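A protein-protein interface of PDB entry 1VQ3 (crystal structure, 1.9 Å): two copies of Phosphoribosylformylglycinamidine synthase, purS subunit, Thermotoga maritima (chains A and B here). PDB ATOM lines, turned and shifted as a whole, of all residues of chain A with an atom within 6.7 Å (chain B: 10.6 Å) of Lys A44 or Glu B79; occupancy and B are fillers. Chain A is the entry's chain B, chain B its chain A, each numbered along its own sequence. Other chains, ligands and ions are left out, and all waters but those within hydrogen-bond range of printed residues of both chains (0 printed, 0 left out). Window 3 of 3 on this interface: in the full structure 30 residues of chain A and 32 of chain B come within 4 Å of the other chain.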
ATOM      1  N   ARG A  38      -0.558  20.539  32.269  1.00  0.00           N
ATOM      2  CA  ARG A  38      -0.930  19.244  32.878  1.00  0.00           C
ATOM      3  C   ARG A  38      -0.564  18.054  31.987  1.00  0.00           C
ATOM      4  O   ARG A  38       0.021  17.065  32.446  1.00  0.00           O
ATOM      5  CB  ARG A  38      -2.415  19.228  33.208  1.00  0.00           C
ATOM      6  CG  ARG A  38      -2.918  17.942  33.898  1.00  0.00           C
ATOM      7  CD  ARG A  38      -4.444  17.922  34.098  1.00  0.00           C
ATOM      8  NE  ARG A  38      -5.221  18.044  32.852  1.00  0.00           N
ATOM      9  CZ  ARG A  38      -5.433  17.049  31.974  1.00  0.00           C
ATOM     10  NH1 ARG A  38      -4.921  15.846  32.181  1.00  0.00           N
ATOM     11  NH2 ARG A  38      -6.164  17.250  30.884  1.00  0.00           N
ATOM     12  N   VAL A  39      -0.922  18.115  30.708  1.00  0.00           N
ATOM     13  CA  VAL A  39      -0.581  17.047  29.812  1.00  0.00           C
ATOM     14  C   VAL A  39       0.930  16.846  29.687  1.00  0.00           C
ATOM     15  O   VAL A  39       1.390  15.689  29.708  1.00  0.00           O
ATOM     16  CB  VAL A  39      -1.138  17.269  28.407  1.00  0.00           C
ATOM     17  CG1 VAL A  39      -0.658  16.144  27.467  1.00  0.00           C
ATOM     18  CG2 VAL A  39      -2.667  17.334  28.464  1.00  0.00           C
ATOM     19  N   LEU A  40       1.682  17.941  29.488  1.00  0.00           N
ATOM     20  CA  LEU A  40       3.121  17.863  29.364  1.00  0.00           C
ATOM     21  C   LEU A  40       3.795  17.302  30.603  1.00  0.00           C
ATOM     22  O   LEU A  40       4.730  16.509  30.495  1.00  0.00           O
ATOM     23  CB  LEU A  40       3.727  19.241  29.078  1.00  0.00           C
ATOM     24  CG  LEU A  40       3.449  19.752  27.671  1.00  0.00           C
ATOM     25  CD1 LEU A  40       3.978  21.166  27.517  1.00  0.00           C
ATOM     26  CD2 LEU A  40       4.062  18.859  26.678  1.00  0.00           C
ATOM     27  N   ARG A  41       3.321  17.685  31.789  1.00  0.00           N
ATOM     28  CA  ARG A  41       3.925  17.175  33.018  1.00  0.00           C
ATOM     29  C   ARG A  41       3.473  15.770  33.343  1.00  0.00           C
ATOM     30  O   ARG A  41       4.297  14.886  33.518  1.00  0.00           O
ATOM     31  CB  ARG A  41       3.583  18.072  34.184  1.00  0.00           C
ATOM     32  CG  ARG A  41       4.208  19.444  34.103  1.00  0.00           C
ATOM     33  CD  ARG A  41       3.783  20.320  35.262  1.00  0.00           C
ATOM     34  NE  ARG A  41       4.335  19.786  36.508  1.00  0.00           N
ATOM     35  CZ  ARG A  41       5.591  19.925  36.891  1.00  0.00           C
ATOM     36  NH1 ARG A  41       6.476  20.573  36.139  1.00  0.00           N
ATOM     37  NH2 ARG A  41       5.981  19.407  38.055  1.00  0.00           N
ATOM     38  N   GLU A  42       2.159  15.567  33.406  1.00  0.00           N
ATOM     39  CA  GLU A  42       1.625  14.303  33.887  1.00  0.00           C
ATOM     40  C   GLU A  42       1.715  13.161  32.899  1.00  0.00           C
ATOM     41  O   GLU A  42       1.999  12.046  33.289  1.00  0.00           O
ATOM     42  CB  GLU A  42       0.201  14.503  34.329  1.00  0.00           C
ATOM     43  CG  GLU A  42       0.124  15.437  35.504  1.00  0.00           C
ATOM     44  CD  GLU A  42      -1.296  15.588  36.034  1.00  0.00           C
ATOM     45  OE1 GLU A  42      -2.189  14.823  35.624  1.00  0.00           O
ATOM     46  OE2 GLU A  42      -1.517  16.491  36.848  1.00  0.00           O
ATOM     47  N   GLU A  43       1.474  13.433  31.625  1.00  0.00           N
ATOM     48  CA  GLU A  43       1.574  12.400  30.635  1.00  0.00           C
ATOM     49  C   GLU A  43       2.939  12.391  29.996  1.00  0.00           C
ATOM     50  O   GLU A  43       3.501  11.322  29.794  1.00  0.00           O
ATOM     51  CB  GLU A  43       0.524  12.544  29.539  1.00  0.00           C
ATOM     52  CG  GLU A  43       0.554  11.383  28.561  1.00  0.00           C
ATOM     53  CD  GLU A  43      -0.113  11.683  27.219  1.00  0.00           C
ATOM     54  OE1 GLU A  43      -1.041  12.521  27.185  1.00  0.00           O
ATOM     55  OE2 GLU A  43       0.299  11.064  26.210  1.00  0.00           O
ATOM     56  N   LYS A  44       3.469  13.550  29.606  1.00  0.00           N
ATOM     57  CA  LYS A  44       4.682  13.496  28.844  1.00  0.00           C
ATOM     58  C   LYS A  44       5.914  13.470  29.729  1.00  0.00           C
ATOM     59  O   LYS A  44       7.020  13.224  29.226  1.00  0.00           O
ATOM     60  CB  LYS A  44       4.763  14.620  27.816  1.00  0.00           C
ATOM     61  CG  LYS A  44       3.542  14.847  26.977  1.00  0.00           C
ATOM     62  CD  LYS A  44       3.128  13.654  26.147  1.00  0.00           C
ATOM     63  CE  LYS A  44       1.961  13.980  25.251  1.00  0.00           C
ATOM     64  NZ  LYS A  44       1.525  12.714  24.576  1.00  0.00           N
ATOM     65  N   GLY A  45       5.740  13.741  31.024  1.00  0.00           N
ATOM     66  CA  GLY A  45       6.845  13.662  31.994  1.00  0.00           C
ATOM     67  C   GLY A  45       7.844  14.806  31.917  1.00  0.00           C
ATOM     68  O   GLY A  45       8.981  14.691  32.394  1.00  0.00           O
ATOM     69  N   LEU A  46       7.431  15.928  31.368  1.00  0.00           N
ATOM     70  CA  LEU A  46       8.358  17.040  31.142  1.00  0.00           C
ATOM     71  C   LEU A  46       8.234  18.055  32.255  1.00  0.00           C
ATOM     72  O   LEU A  46       7.095  18.451  32.592  1.00  0.00           O
ATOM     73  CB  LEU A  46       8.073  17.706  29.816  1.00  0.00           C
ATOM     74  CG  LEU A  46       8.283  16.796  28.587  1.00  0.00           C
ATOM     75  CD1 LEU A  46       7.980  17.516  27.304  1.00  0.00           C
ATOM     76  CD2 LEU A  46       9.714  16.169  28.562  1.00  0.00           C
ATOM     77  N   ILE B  20       7.989  29.968  22.511  1.00  0.00           N
ATOM     78  CA  ILE B  20       7.902  29.152  21.272  1.00  0.00           C
ATOM     79  C   ILE B  20       6.971  29.882  20.345  1.00  0.00           C
ATOM     80  O   ILE B  20       5.814  30.137  20.681  1.00  0.00           O
ATOM     81  CB  ILE B  20       7.349  27.745  21.619  1.00  0.00           C
ATOM     82  CG1 ILE B  20       8.195  27.094  22.735  1.00  0.00           C
ATOM     83  CG2 ILE B  20       7.384  26.825  20.397  1.00  0.00           C
ATOM     84  CD1 ILE B  20       7.540  25.946  23.427  1.00  0.00           C
ATOM     85  N   ILE B  57       3.817  30.379  22.715  1.00  0.00           N
ATOM     86  CA  ILE B  57       3.699  29.623  23.956  1.00  0.00           C
ATOM     87  C   ILE B  57       4.863  30.078  24.824  1.00  0.00           C
ATOM     88  O   ILE B  57       6.015  30.026  24.388  1.00  0.00           O
ATOM     89  CB  ILE B  57       3.689  28.090  23.696  1.00  0.00           C
ATOM     90  CG1 ILE B  57       2.463  27.732  22.832  1.00  0.00           C
ATOM     91  CG2 ILE B  57       3.709  27.352  25.059  1.00  0.00           C
ATOM     92  CD1 ILE B  57       2.444  26.333  22.189  1.00  0.00           C
ATOM     93  N   GLU B  71      16.419  21.186  25.425  1.00  0.00           N
ATOM     94  CA  GLU B  71      16.106  19.872  24.887  1.00  0.00           C
ATOM     95  C   GLU B  71      14.679  19.520  25.279  1.00  0.00           C
ATOM     96  O   GLU B  71      13.910  18.952  24.454  1.00  0.00           O
ATOM     97  CB  GLU B  71      17.096  18.811  25.408  1.00  0.00           C
ATOM     98  CG  GLU B  71      18.521  18.865  24.800  1.00  0.00           C
ATOM     99  CD  GLU B  71      18.566  18.974  23.265  1.00  0.00           C
ATOM    100  OE1 GLU B  71      18.120  18.043  22.558  1.00  0.00           O
ATOM    101  OE2 GLU B  71      19.067  19.994  22.744  1.00  0.00           O
ATOM    102  N   ILE B  72      14.326  19.860  26.516  1.00  0.00           N
ATOM    103  CA  ILE B  72      12.951  19.641  27.036  1.00  0.00           C
ATOM    104  C   ILE B  72      11.909  20.442  26.235  1.00  0.00           C
ATOM    105  O   ILE B  72      10.847  19.942  25.885  1.00  0.00           O
ATOM    106  CB  ILE B  72      12.858  19.958  28.528  1.00  0.00           C
ATOM    107  CG1 ILE B  72      13.680  18.973  29.372  1.00  0.00           C
ATOM    108  CG2 ILE B  72      11.394  19.933  29.005  1.00  0.00           C
ATOM    109  CD1 ILE B  72      14.081  19.535  30.763  1.00  0.00           C
ATOM    110  N   VAL B  73      12.209  21.699  25.961  1.00  0.00           N
ATOM    111  CA  VAL B  73      11.331  22.504  25.107  1.00  0.00           C
ATOM    112  C   VAL B  73      11.095  21.796  23.771  1.00  0.00           C
ATOM    113  O   VAL B  73       9.952  21.674  23.300  1.00  0.00           O
ATOM    114  CB  VAL B  73      11.884  23.969  24.901  1.00  0.00           C
ATOM    115  CG1 VAL B  73      11.085  24.741  23.834  1.00  0.00           C
ATOM    116  CG2 VAL B  73      11.887  24.715  26.239  1.00  0.00           C
ATOM    117  N   LYS B  74      12.145  21.328  23.135  1.00  0.00           N
ATOM    118  CA  LYS B  74      11.993  20.706  21.821  1.00  0.00           C
ATOM    119  C   LYS B  74      11.151  19.427  21.931  1.00  0.00           C
ATOM    120  O   LYS B  74      10.333  19.106  21.075  1.00  0.00           O
ATOM    121  CB  LYS B  74      13.359  20.337  21.230  1.00  0.00           C
ATOM    122  CG  LYS B  74      14.137  21.512  20.665  1.00  0.00           C
ATOM    123  CD  LYS B  74      15.425  21.031  19.944  1.00  0.00           C
ATOM    124  CE  LYS B  74      16.469  20.463  20.889  1.00  0.00           C
ATOM    125  NZ  LYS B  74      17.681  19.887  20.153  1.00  0.00           N
ATOM    126  N   LYS B  75      11.395  18.679  22.987  1.00  0.00           N
ATOM    127  CA  LYS B  75      10.597  17.495  23.261  1.00  0.00           C
ATOM    128  C   LYS B  75       9.117  17.866  23.466  1.00  0.00           C
ATOM    129  O   LYS B  75       8.250  17.206  22.943  1.00  0.00           O
ATOM    130  CB  LYS B  75      11.142  16.765  24.496  1.00  0.00           C
ATOM    131  CG  LYS B  75      10.535  15.395  24.753  1.00  0.00           C
ATOM    132  N   ALA B  76       8.828  18.932  24.215  1.00  0.00           N
ATOM    133  CA  ALA B  76       7.450  19.435  24.344  1.00  0.00           C
ATOM    134  C   ALA B  76       6.794  19.794  22.998  1.00  0.00           C
ATOM    135  O   ALA B  76       5.616  19.458  22.735  1.00  0.00           O
ATOM    136  CB  ALA B  76       7.420  20.603  25.290  1.00  0.00           C
ATOM    137  N   CYS B  77       7.579  20.396  22.112  1.00  0.00           N
ATOM    138  CA  CYS B  77       7.114  20.682  20.741  1.00  0.00           C
ATOM    139  C   CYS B  77       6.802  19.415  19.938  1.00  0.00           C
ATOM    140  O   CYS B  77       5.743  19.303  19.354  1.00  0.00           O
ATOM    141  CB  CYS B  77       8.123  21.562  20.014  1.00  0.00           C
ATOM    142  SG  CYS B  77       8.240  23.175  20.827  1.00  0.00           S
ATOM    143  N   GLU B  78       7.709  18.455  19.995  1.00  0.00           N
ATOM    144  CA  GLU B  78       7.562  17.178  19.285  1.00  0.00           C
ATOM    145  C   GLU B  78       6.386  16.390  19.823  1.00  0.00           C
ATOM    146  O   GLU B  78       5.618  15.785  19.069  1.00  0.00           O
ATOM    147  CB  GLU B  78       8.833  16.344  19.461  1.00  0.00           C
ATOM    148  CG  GLU B  78       9.939  16.830  18.590  1.00  0.00           C
ATOM    149  CD  GLU B  78      11.256  16.134  18.840  1.00  0.00           C
ATOM    150  OE1 GLU B  78      11.373  15.350  19.831  1.00  0.00           O
ATOM    151  OE2 GLU B  78      12.175  16.414  18.051  1.00  0.00           O
ATOM    152  N   GLU B  79       6.238  16.388  21.134  1.00  0.00           N
ATOM    153  CA  GLU B  79       5.223  15.554  21.753  1.00  0.00           C
ATOM    154  C   GLU B  79       3.856  16.178  21.757  1.00  0.00           C
ATOM    155  O   GLU B  79       2.876  15.470  21.910  1.00  0.00           O
ATOM    156  CB  GLU B  79       5.601  15.192  23.183  1.00  0.00           C
ATOM    157  CG  GLU B  79       6.859  14.330  23.250  1.00  0.00           C
ATOM    158  CD  GLU B  79       6.776  13.118  22.346  1.00  0.00           C
ATOM    159  OE1 GLU B  79       5.718  12.443  22.330  1.00  0.00           O
ATOM    160  OE2 GLU B  79       7.768  12.840  21.632  1.00  0.00           O
ATOM    161  N   LEU B  80       3.755  17.487  21.605  1.00  0.00           N
ATOM    162  CA  LEU B  80       2.434  18.087  21.764  1.00  0.00           C
ATOM    163  C   LEU B  80       2.239  19.467  21.145  1.00  0.00           C
ATOM    164  O   LEU B  80       1.155  19.769  20.636  1.00  0.00           O
ATOM    165  CB  LEU B  80       2.109  18.155  23.236  1.00  0.00           C
ATOM    166  CG  LEU B  80       0.705  18.669  23.629  1.00  0.00           C
ATOM    167  CD1 LEU B  80      -0.362  17.654  23.223  1.00  0.00           C
ATOM    168  CD2 LEU B  80       0.596  18.979  25.099  1.00  0.00           C
ATOM    169  N   LEU B  81       3.222  20.359  21.274  1.00  0.00           N
ATOM    170  CA  LEU B  81       2.935  21.765  21.011  1.00  0.00           C
ATOM    171  C   LEU B  81       2.936  22.164  19.547  1.00  0.00           C
ATOM    172  O   LEU B  81       2.316  23.168  19.200  1.00  0.00           O
ATOM    173  CB  LEU B  81       3.896  22.684  21.827  1.00  0.00           C
ATOM    174  CG  LEU B  81       3.961  22.391  23.340  1.00  0.00           C
ATOM    175  CD1 LEU B  81       4.983  23.402  23.882  1.00  0.00           C
ATOM    176  CD2 LEU B  81       2.601  22.547  23.957  1.00  0.00           C
ATOM    177  N   VAL B  82       3.586  21.362  18.705  1.00  0.00           N
ATOM    178  CA  VAL B  82       3.767  21.683  17.310  1.00  0.00           C
ATOM    179  C   VAL B  82       3.322  20.485  16.466  1.00  0.00           C
ATOM    180  O   VAL B  82       3.742  19.377  16.686  1.00  0.00           O
ATOM    181  CB  VAL B  82       5.195  22.084  17.012  1.00  0.00           C
ATOM    182  CG1 VAL B  82       5.352  22.565  15.649  1.00  0.00           C
ATOM    183  CG2 VAL B  82       5.622  23.228  17.946  1.00  0.00           C
ATOM    184  N   ASN B  83       2.450  20.765  15.529  1.00  0.00           N
ATOM    185  CA  ASN B  83       1.993  19.795  14.529  1.00  0.00           C
ATOM    186  C   ASN B  83       3.042  19.627  13.455  1.00  0.00           C
ATOM    187  O   ASN B  83       3.376  20.583  12.746  1.00  0.00           O
ATOM    188  CB  ASN B  83       0.672  20.287  13.916  1.00  0.00           C
ATOM    189  CG  ASN B  83      -0.038  19.219  13.096  1.00  0.00           C
ATOM    190  OD1 ASN B  83       0.548  18.574  12.242  1.00  0.00           O
ATOM    191  ND2 ASN B  83      -1.335  19.053  13.355  1.00  0.00           N
ATOM    192  N   PRO B  84       3.588  18.427  13.354  1.00  0.00           N
ATOM    193  CA  PRO B  84       4.705  18.183  12.498  1.00  0.00           C
ATOM    194  C   PRO B  84       4.373  18.229  11.027  1.00  0.00           C
ATOM    195  O   PRO B  84       5.265  18.407  10.232  1.00  0.00           O
ATOM    196  CB  PRO B  84       5.128  16.757  12.868  1.00  0.00           C
ATOM    197  CG  PRO B  84       3.972  16.139  13.337  1.00  0.00           C
ATOM    198  CD  PRO B  84       3.194  17.212  14.081  1.00  0.00           C
ATOM    199  N   GLU B  87       2.945  22.633  10.733  1.00  0.00           N
ATOM    200  CA  GLU B  87       3.591  23.739  11.509  1.00  0.00           C
ATOM    201  C   GLU B  87       5.112  23.677  11.574  1.00  0.00           C
ATOM    202  O   GLU B  87       5.717  22.612  11.367  1.00  0.00           O
ATOM    203  CB  GLU B  87       3.011  23.826  12.926  1.00  0.00           C
ATOM    204  CG  GLU B  87       1.624  24.495  12.967  1.00  0.00           C
ATOM    205  CD  GLU B  87       0.931  24.366  14.323  1.00  0.00           C
ATOM    206  OE1 GLU B  87       1.252  23.462  15.115  1.00  0.00           O
ATOM    207  OE2 GLU B  87       0.071  25.202  14.609  1.00  0.00           O
ATOM    208  N   TYR B  89       8.427  25.865  13.946  1.00  0.00           N
ATOM    209  CA  TYR B  89       8.569  26.604  15.193  1.00  0.00           C
ATOM    210  C   TYR B  89       9.957  27.180  15.429  1.00  0.00           C
ATOM    211  O   TYR B  89      10.950  26.608  15.002  1.00  0.00           O
ATOM    212  CB  TYR B  89       8.099  25.721  16.354  1.00  0.00           C
ATOM    213  CG  TYR B  89       9.053  24.610  16.789  1.00  0.00           C
ATOM    214  CD1 TYR B  89       9.172  23.426  16.052  1.00  0.00           C
ATOM    215  CD2 TYR B  89       9.858  24.751  17.919  1.00  0.00           C
ATOM    216  CE1 TYR B  89      10.021  22.450  16.435  1.00  0.00           C
ATOM    217  CE2 TYR B  89      10.682  23.733  18.324  1.00  0.00           C
ATOM    218  CZ  TYR B  89      10.755  22.602  17.598  1.00  0.00           C
ATOM    219  OH  TYR B  89      11.573  21.600  18.013  1.00  0.00           O
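O of Ala B76 lies within hydrogen-bond range of N of Leu B81 (2.9 Å). The backbone carbonyl oxygen of Leu A40 sits at hydrogen-bond distance from the backbone NH of Gly A45 (3.0 Å). O of Leu A40 sits at hydrogen-bond distance from N of Leu A46, at 2.9 Å. N of Lys A44 sits at hydrogen-bond distance from O of Val A39 (3.0 Å). The side-chain carboxylate (OE2) of Glu A43 lies within salt-bridge range of the side-chain amino group (NZ) of Lys A44 (2.6 Å).
Leu B80 touches Val A39 (CD2 to CG1, 3.9 Å). Leu B80 touches Leu A40 (CD2 to CD2, 3.8 Å). CE of Lys A44 touches O of Glu B79 (3.8 Å). CD2 of Leu A46 touches CG of Lys B75, at 3.97 Å. N of Ala B76 touches CD1 of Leu A46, 3.5 Å away.
Printed residues of chain B within 4 Å of Val A39: Leu B80 (3.9 Å). Leu A40 touches just one residue of chain B: Leu B80. No residue of chain B comes within 4 Å of Glu A43. Of chain B, only Glu B79 (3.8 Å) comes within 4 Å of Lys A44. No residue of chain B comes within 4 Å of Gly A45. Of the printed residues of chain B, Leu A46 touches Lys B75 (3.97 Å) and Ala B76 (3.5 Å). Of the printed residues of chain A, Lys B75 touches Leu A46. Printed residues of chain A within 4 Å of Ala B76: Leu A46. Of chain A, only Lys A44 (3.8 Å) comes within 4 Å of Glu B79. Printed residues of chain A within 4 Å of Leu B80: Val A39 and Leu A40.
Of the 18 printed residues of chain B, 4 touch a printed residue of chain A. Printed residues of chain B that touch a printed residue of chain A: Lys B75, Ala B76, Glu B79 and Leu B80. Hydrophobic or aromatic side chains of chain B that line the printed part of chain A: Ala B76 and Leu B80. Along chain B the printed residues that touch a printed residue of chain A span positions 75 to 80.
No position is printed for both chains. Of the 5 pairs that touch across the chains among the printed residues, none has its exchanged pair printed and touching as well.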
